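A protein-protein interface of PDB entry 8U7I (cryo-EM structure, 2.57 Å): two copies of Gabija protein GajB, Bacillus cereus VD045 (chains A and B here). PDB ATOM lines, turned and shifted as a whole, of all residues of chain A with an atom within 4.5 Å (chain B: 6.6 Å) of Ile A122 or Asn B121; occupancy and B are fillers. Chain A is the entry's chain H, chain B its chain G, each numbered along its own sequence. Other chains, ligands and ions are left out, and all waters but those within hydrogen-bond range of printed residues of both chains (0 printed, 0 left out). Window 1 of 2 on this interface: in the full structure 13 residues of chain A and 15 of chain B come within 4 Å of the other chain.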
ATOM      1  N   PHE A  98      27.523   7.070  -1.156  1.00  0.00           N
ATOM      2  CA  PHE A  98      26.275   7.242  -0.435  1.00  0.00           C
ATOM      3  C   PHE A  98      25.652   8.602  -0.751  1.00  0.00           C
ATOM      4  O   PHE A  98      26.286   9.499  -1.313  1.00  0.00           O
ATOM      5  CB  PHE A  98      26.511   7.113   1.067  1.00  0.00           C
ATOM      6  CG  PHE A  98      27.438   8.156   1.623  1.00  0.00           C
ATOM      7  CD1 PHE A  98      28.810   8.022   1.498  1.00  0.00           C
ATOM      8  CD2 PHE A  98      26.938   9.276   2.262  1.00  0.00           C
ATOM      9  CE1 PHE A  98      29.662   8.981   2.002  1.00  0.00           C
ATOM     10  CE2 PHE A  98      27.786  10.236   2.770  1.00  0.00           C
ATOM     11  CZ  PHE A  98      29.150  10.090   2.637  1.00  0.00           C
ATOM     12  N   THR A  99      24.385   8.745  -0.371  1.00  0.00           N
ATOM     13  CA  THR A  99      23.641   9.981  -0.551  1.00  0.00           C
ATOM     14  C   THR A  99      22.900  10.299   0.739  1.00  0.00           C
ATOM     15  O   THR A  99      22.597   9.404   1.531  1.00  0.00           O
ATOM     16  CB  THR A  99      22.653   9.876  -1.722  1.00  0.00           C
ATOM     17  OG1 THR A  99      23.266   9.161  -2.802  1.00  0.00           O
ATOM     18  CG2 THR A  99      22.253  11.258  -2.214  1.00  0.00           C
ATOM     19  N   LEU A 117      23.525   1.152   7.741  1.00  0.00           N
ATOM     20  CA  LEU A 117      24.296   1.929   6.778  1.00  0.00           C
ATOM     21  C   LEU A 117      25.192   1.031   5.934  1.00  0.00           C
ATOM     22  O   LEU A 117      25.383   1.282   4.739  1.00  0.00           O
ATOM     23  CB  LEU A 117      25.124   2.989   7.505  1.00  0.00           C
ATOM     24  CG  LEU A 117      26.307   3.597   6.748  1.00  0.00           C
ATOM     25  CD1 LEU A 117      25.833   4.436   5.570  1.00  0.00           C
ATOM     26  CD2 LEU A 117      27.171   4.423   7.684  1.00  0.00           C
ATOM     27  N   GLN A 120      22.410  -0.867   3.642  1.00  0.00           N
ATOM     28  CA  GLN A 120      21.647   0.045   2.798  1.00  0.00           C
ATOM     29  C   GLN A 120      22.558   0.907   1.935  1.00  0.00           C
ATOM     30  O   GLN A 120      22.153   1.332   0.846  1.00  0.00           O
ATOM     31  CB  GLN A 120      20.734   0.924   3.653  1.00  0.00           C
ATOM     32  CG  GLN A 120      19.826   1.844   2.854  1.00  0.00           C
ATOM     33  CD  GLN A 120      18.882   1.085   1.941  1.00  0.00           C
ATOM     34  OE1 GLN A 120      18.882   1.284   0.727  1.00  0.00           O
ATOM     35  NE2 GLN A 120      18.074   0.209   2.523  1.00  0.00           N
ATOM     36  N   ASN A 121      23.776   1.176   2.404  1.00  0.00           N
ATOM     37  CA  ASN A 121      24.825   1.891   1.682  1.00  0.00           C
ATOM     38  C   ASN A 121      24.504   3.359   1.444  1.00  0.00           C
ATOM     39  O   ASN A 121      25.216   4.020   0.678  1.00  0.00           O
ATOM     40  CB  ASN A 121      25.147   1.227   0.337  1.00  0.00           C
ATOM     41  CG  ASN A 121      25.721  -0.166   0.497  1.00  0.00           C
ATOM     42  OD1 ASN A 121      25.220  -0.969   1.281  1.00  0.00           O
ATOM     43  ND2 ASN A 121      26.779  -0.460  -0.249  1.00  0.00           N
ATOM     44  N   ILE A 122      23.453   3.894   2.062  1.00  0.00           N
ATOM     45  CA  ILE A 122      23.044   5.280   1.863  1.00  0.00           C
ATOM     46  C   ILE A 122      22.896   5.951   3.219  1.00  0.00           C
ATOM     47  O   ILE A 122      22.271   5.395   4.130  1.00  0.00           O
ATOM     48  CB  ILE A 122      21.736   5.390   1.054  1.00  0.00           C
ATOM     49  CG1 ILE A 122      22.020   5.342  -0.449  1.00  0.00           C
ATOM     50  CG2 ILE A 122      20.977   6.661   1.402  1.00  0.00           C
ATOM     51  CD1 ILE A 122      22.484   4.009  -0.981  1.00  0.00           C
ATOM     52  N   LEU A 123      23.474   7.143   3.352  1.00  0.00           N
ATOM     53  CA  LEU A 123      23.394   7.890   4.596  1.00  0.00           C
ATOM     54  C   LEU A 123      21.999   8.467   4.798  1.00  0.00           C
ATOM     55  O   LEU A 123      21.304   8.830   3.845  1.00  0.00           O
ATOM     56  CB  LEU A 123      24.426   9.019   4.607  1.00  0.00           C
ATOM     57  CG  LEU A 123      24.712   9.686   5.954  1.00  0.00           C
ATOM     58  CD1 LEU A 123      24.811   8.651   7.062  1.00  0.00           C
ATOM     59  CD2 LEU A 123      25.981  10.516   5.877  1.00  0.00           C
ATOM     60  N   GLY A 124      21.592   8.549   6.063  1.00  0.00           N
ATOM     61  CA  GLY A 124      20.326   9.148   6.426  1.00  0.00           C
ATOM     62  C   GLY A 124      20.462   9.918   7.724  1.00  0.00           C
ATOM     63  O   GLY A 124      21.546  10.008   8.303  1.00  0.00           O
ATOM     64  N   PRO B  95      18.649   7.832  -8.881  1.00  0.00           N
ATOM     65  CA  PRO B  95      20.092   8.057  -8.815  1.00  0.00           C
ATOM     66  C   PRO B  95      20.851   7.318  -9.909  1.00  0.00           C
ATOM     67  O   PRO B  95      20.371   6.354 -10.507  1.00  0.00           O
ATOM     68  CB  PRO B  95      20.457   7.500  -7.434  1.00  0.00           C
ATOM     69  CG  PRO B  95      19.426   6.421  -7.181  1.00  0.00           C
ATOM     70  CD  PRO B  95      18.243   6.657  -8.093  1.00  0.00           C
ATOM     71  N   ASP B  96      22.068   7.799 -10.159  1.00  0.00           N
ATOM     72  CA  ASP B  96      22.972   7.183 -11.117  1.00  0.00           C
ATOM     73  C   ASP B  96      24.296   6.759 -10.499  1.00  0.00           C
ATOM     74  O   ASP B  96      25.214   6.381 -11.232  1.00  0.00           O
ATOM     75  CB  ASP B  96      23.228   8.135 -12.292  1.00  0.00           C
ATOM     76  CG  ASP B  96      23.992   9.383 -11.884  1.00  0.00           C
ATOM     77  OD1 ASP B  96      24.172   9.617 -10.671  1.00  0.00           O
ATOM     78  OD2 ASP B  96      24.418  10.133 -12.786  1.00  0.00           O
ATOM     79  N   ASN B  97      24.426   6.830  -9.175  1.00  0.00           N
ATOM     80  CA  ASN B  97      25.639   6.426  -8.481  1.00  0.00           C
ATOM     81  C   ASN B  97      25.408   5.237  -7.556  1.00  0.00           C
ATOM     82  O   ASN B  97      26.219   4.989  -6.658  1.00  0.00           O
ATOM     83  CB  ASN B  97      26.214   7.608  -7.699  1.00  0.00           C
ATOM     84  CG  ASN B  97      25.464   7.874  -6.410  1.00  0.00           C
ATOM     85  OD1 ASN B  97      24.235   7.818  -6.370  1.00  0.00           O
ATOM     86  ND2 ASN B  97      26.202   8.169  -5.347  1.00  0.00           N
ATOM     87  N   PHE B  98      24.325   4.493  -7.765  1.00  0.00           N
ATOM     88  CA  PHE B  98      23.996   3.381  -6.890  1.00  0.00           C
ATOM     89  C   PHE B  98      24.991   2.234  -7.068  1.00  0.00           C
ATOM     90  O   PHE B  98      25.898   2.276  -7.904  1.00  0.00           O
ATOM     91  CB  PHE B  98      22.560   2.914  -7.141  1.00  0.00           C
ATOM     92  CG  PHE B  98      22.251   2.595  -8.579  1.00  0.00           C
ATOM     93  CD1 PHE B  98      22.906   1.575  -9.248  1.00  0.00           C
ATOM     94  CD2 PHE B  98      21.288   3.317  -9.260  1.00  0.00           C
ATOM     95  CE1 PHE B  98      22.609   1.285 -10.561  1.00  0.00           C
ATOM     96  CE2 PHE B  98      20.991   3.033 -10.576  1.00  0.00           C
ATOM     97  CZ  PHE B  98      21.654   2.017 -11.226  1.00  0.00           C
ATOM     98  N   THR B  99      24.803   1.193  -6.263  1.00  0.00           N
ATOM     99  CA  THR B  99      25.657   0.014  -6.275  1.00  0.00           C
ATOM    100  C   THR B  99      24.784  -1.230  -6.350  1.00  0.00           C
ATOM    101  O   THR B  99      23.724  -1.292  -5.720  1.00  0.00           O
ATOM    102  CB  THR B  99      26.551  -0.033  -5.027  1.00  0.00           C
ATOM    103  OG1 THR B  99      27.375   1.138  -4.985  1.00  0.00           O
ATOM    104  CG2 THR B  99      27.444  -1.264  -5.044  1.00  0.00           C
ATOM    105  N   VAL B 116      11.083   0.552  -4.810  1.00  0.00           N
ATOM    106  CA  VAL B 116      12.155   0.594  -3.820  1.00  0.00           C
ATOM    107  C   VAL B 116      13.413   1.202  -4.423  1.00  0.00           C
ATOM    108  O   VAL B 116      14.248   1.754  -3.700  1.00  0.00           O
ATOM    109  CB  VAL B 116      12.440  -0.806  -3.242  1.00  0.00           C
ATOM    110  CG1 VAL B 116      11.221  -1.354  -2.518  1.00  0.00           C
ATOM    111  CG2 VAL B 116      12.911  -1.759  -4.327  1.00  0.00           C
ATOM    112  N   LEU B 117      13.560   1.128  -5.749  1.00  0.00           N
ATOM    113  CA  LEU B 117      14.808   1.532  -6.388  1.00  0.00           C
ATOM    114  C   LEU B 117      15.107   3.009  -6.163  1.00  0.00           C
ATOM    115  O   LEU B 117      16.258   3.383  -5.908  1.00  0.00           O
ATOM    116  CB  LEU B 117      14.750   1.219  -7.884  1.00  0.00           C
ATOM    117  CG  LEU B 117      15.844   1.824  -8.767  1.00  0.00           C
ATOM    118  CD1 LEU B 117      17.229   1.372  -8.327  1.00  0.00           C
ATOM    119  CD2 LEU B 117      15.602   1.474 -10.224  1.00  0.00           C
ATOM    120  N   LYS B 118      14.088   3.864  -6.260  1.00  0.00           N
ATOM    121  CA  LYS B 118      14.314   5.297  -6.110  1.00  0.00           C
ATOM    122  C   LYS B 118      14.820   5.635  -4.713  1.00  0.00           C
ATOM    123  O   LYS B 118      15.790   6.385  -4.557  1.00  0.00           O
ATOM    124  CB  LYS B 118      13.028   6.062  -6.420  1.00  0.00           C
ATOM    125  CG  LYS B 118      13.138   7.565  -6.229  1.00  0.00           C
ATOM    126  CD  LYS B 118      11.767   8.208  -6.106  1.00  0.00           C
ATOM    127  CE  LYS B 118      10.813   7.692  -7.170  1.00  0.00           C
ATOM    128  NZ  LYS B 118       9.674   8.623  -7.391  1.00  0.00           N
ATOM    129  N   TYR B 119      14.179   5.082  -3.682  1.00  0.00           N
ATOM    130  CA  TYR B 119      14.554   5.406  -2.311  1.00  0.00           C
ATOM    131  C   TYR B 119      15.821   4.689  -1.862  1.00  0.00           C
ATOM    132  O   TYR B 119      16.629   5.273  -1.132  1.00  0.00           O
ATOM    133  CB  TYR B 119      13.404   5.077  -1.358  1.00  0.00           C
ATOM    134  CG  TYR B 119      12.034   5.389  -1.916  1.00  0.00           C
ATOM    135  CD1 TYR B 119      11.754   6.632  -2.465  1.00  0.00           C
ATOM    136  CD2 TYR B 119      11.019   4.445  -1.885  1.00  0.00           C
ATOM    137  CE1 TYR B 119      10.505   6.926  -2.972  1.00  0.00           C
ATOM    138  CE2 TYR B 119       9.766   4.731  -2.389  1.00  0.00           C
ATOM    139  CZ  TYR B 119       9.515   5.971  -2.932  1.00  0.00           C
ATOM    140  OH  TYR B 119       8.268   6.259  -3.436  1.00  0.00           O
ATOM    141  N   GLN B 120      16.015   3.436  -2.280  1.00  0.00           N
ATOM    142  CA  GLN B 120      17.130   2.653  -1.761  1.00  0.00           C
ATOM    143  C   GLN B 120      18.479   3.146  -2.271  1.00  0.00           C
ATOM    144  O   GLN B 120      19.473   3.066  -1.540  1.00  0.00           O
ATOM    145  CB  GLN B 120      16.941   1.172  -2.104  1.00  0.00           C
ATOM    146  CG  GLN B 120      17.207   0.811  -3.555  1.00  0.00           C
ATOM    147  CD  GLN B 120      16.893  -0.638  -3.862  1.00  0.00           C
ATOM    148  OE1 GLN B 120      16.278  -0.949  -4.881  1.00  0.00           O
ATOM    149  NE2 GLN B 120      17.310  -1.535  -2.978  1.00  0.00           N
ATOM    150  N   ASN B 121      18.536   3.652  -3.506  1.00  0.00           N
ATOM    151  CA  ASN B 121      19.776   4.141  -4.113  1.00  0.00           C
ATOM    152  C   ASN B 121      20.849   3.053  -4.160  1.00  0.00           C
ATOM    153  O   ASN B 121      22.047   3.341  -4.086  1.00  0.00           O
ATOM    154  CB  ASN B 121      20.285   5.394  -3.390  1.00  0.00           C
ATOM    155  CG  ASN B 121      21.317   6.179  -4.195  1.00  0.00           C
ATOM    156  OD1 ASN B 121      21.606   7.334  -3.881  1.00  0.00           O
ATOM    157  ND2 ASN B 121      21.888   5.553  -5.217  1.00  0.00           N
ATOM    158  N   ILE B 122      20.427   1.795  -4.268  1.00  0.00           N
ATOM    159  CA  ILE B 122      21.297   0.687  -4.639  1.00  0.00           C
ATOM    160  C   ILE B 122      20.560  -0.144  -5.677  1.00  0.00           C
ATOM    161  O   ILE B 122      19.330  -0.256  -5.649  1.00  0.00           O
ATOM    162  CB  ILE B 122      21.722  -0.188  -3.433  1.00  0.00           C
ATOM    163  CG1 ILE B 122      20.537  -0.983  -2.885  1.00  0.00           C
ATOM    164  CG2 ILE B 122      22.371   0.652  -2.344  1.00  0.00           C
ATOM    165  CD1 ILE B 122      20.871  -1.795  -1.656  1.00  0.00           C
ATOM    166  N   LEU B 123      21.312  -0.713  -6.615  1.00  0.00           N
ATOM    167  CA  LEU B 123      20.702  -1.468  -7.704  1.00  0.00           C
ATOM    168  C   LEU B 123      20.206  -2.799  -7.157  1.00  0.00           C
ATOM    169  O   LEU B 123      20.994  -3.727  -6.945  1.00  0.00           O
ATOM    170  CB  LEU B 123      21.689  -1.672  -8.847  1.00  0.00           C
ATOM    171  CG  LEU B 123      21.141  -2.441 -10.051  1.00  0.00           C
ATOM    172  CD1 LEU B 123      19.783  -1.897 -10.471  1.00  0.00           C
ATOM    173  CD2 LEU B 123      22.117  -2.367 -11.205  1.00  0.00           C
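The side-chain amide oxygen (OD1) of Asn B121 is in hydrogen-bond range of the side-chain hydroxyl (OG1) of Thr A99 (2.7 Å).
The backbone carbonyl oxygen (O) of Gln B120 sits close to the side-chain amide oxygen (OE1) of Gln A120, 2.9 Å away.
The side-chain amide nitrogen (ND2) of Asn B121 sits at hydrogen-bond distance from the side-chain amide oxygen (OD1) of Asn B97 (3.5 Å).
The backbone carbonyl oxygen of Thr A99 lies within hydrogen-bond range of the backbone NH of Leu A123 (3.0 Å).
The side-chain amide oxygen of Gln B120 sits close to the backbone carbonyl oxygen of Ile B122 (3.2 Å).
Among the printed residues, pairs that only touch across the chains: Ile A122 with Gln B120, Ile A122 with Asn B121, Gln A120 with Ile B122, Ile A122 with Ile B122, Asn A121 with Ile B122 and Thr A99 with Asn B97.
Leu A117 touches none of the printed residues of chain B.
Printed residues of chain B within 4 Å of Gln A120: Gln B120 (2.9 Å) and Ile B122 (3.3 Å).
Of the printed residues of chain B, Asn A121 touches Ile B122 (3.9 Å).
Ile A122 touches just these residues of chain B: Gln B120, Asn B121 and Ile B122.
Gly A124 touches none of the printed residues of chain B.
Of the printed residues of chain A, Asn B97 touches Thr A99.
Asn B121 touches just these residues of chain A: Thr A99 (2.7 Å) and Ile A122 (3.2 Å).
Of the printed residues of chain A, Ile B122 touches Gln A120, Asn A121 and Ile A122.
The nearest printed residue of chain A that does not touch Asn B121 is Gln A120 (4.9 Å).
Of the 8 printed residues of chain A, 4 touch a printed residue of chain B.
Of the 13 printed residues of chain B, 4 touch a printed residue of chain A.
Hydrophobic or aromatic side chains of chain B that line the printed part of chain A: Ile B122.
Among the printed residues, 8 pairs touch across the chains.
Among the printed residues, no Asp or Glu carboxylate lies within 4 Å of a Lys or Arg side-chain nitrogen of the other chain.
Gln B120 touches its own counterpart, Gln A120.
Gln A120 touches Ile B122, and with the chains exchanged Ile A122 touches Gln B120.
Asn A121 touches Ile B122, and with the chains exchanged Ile A122 touches Asn B121.
Ile A122 touches its own counterpart, Ile B122.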
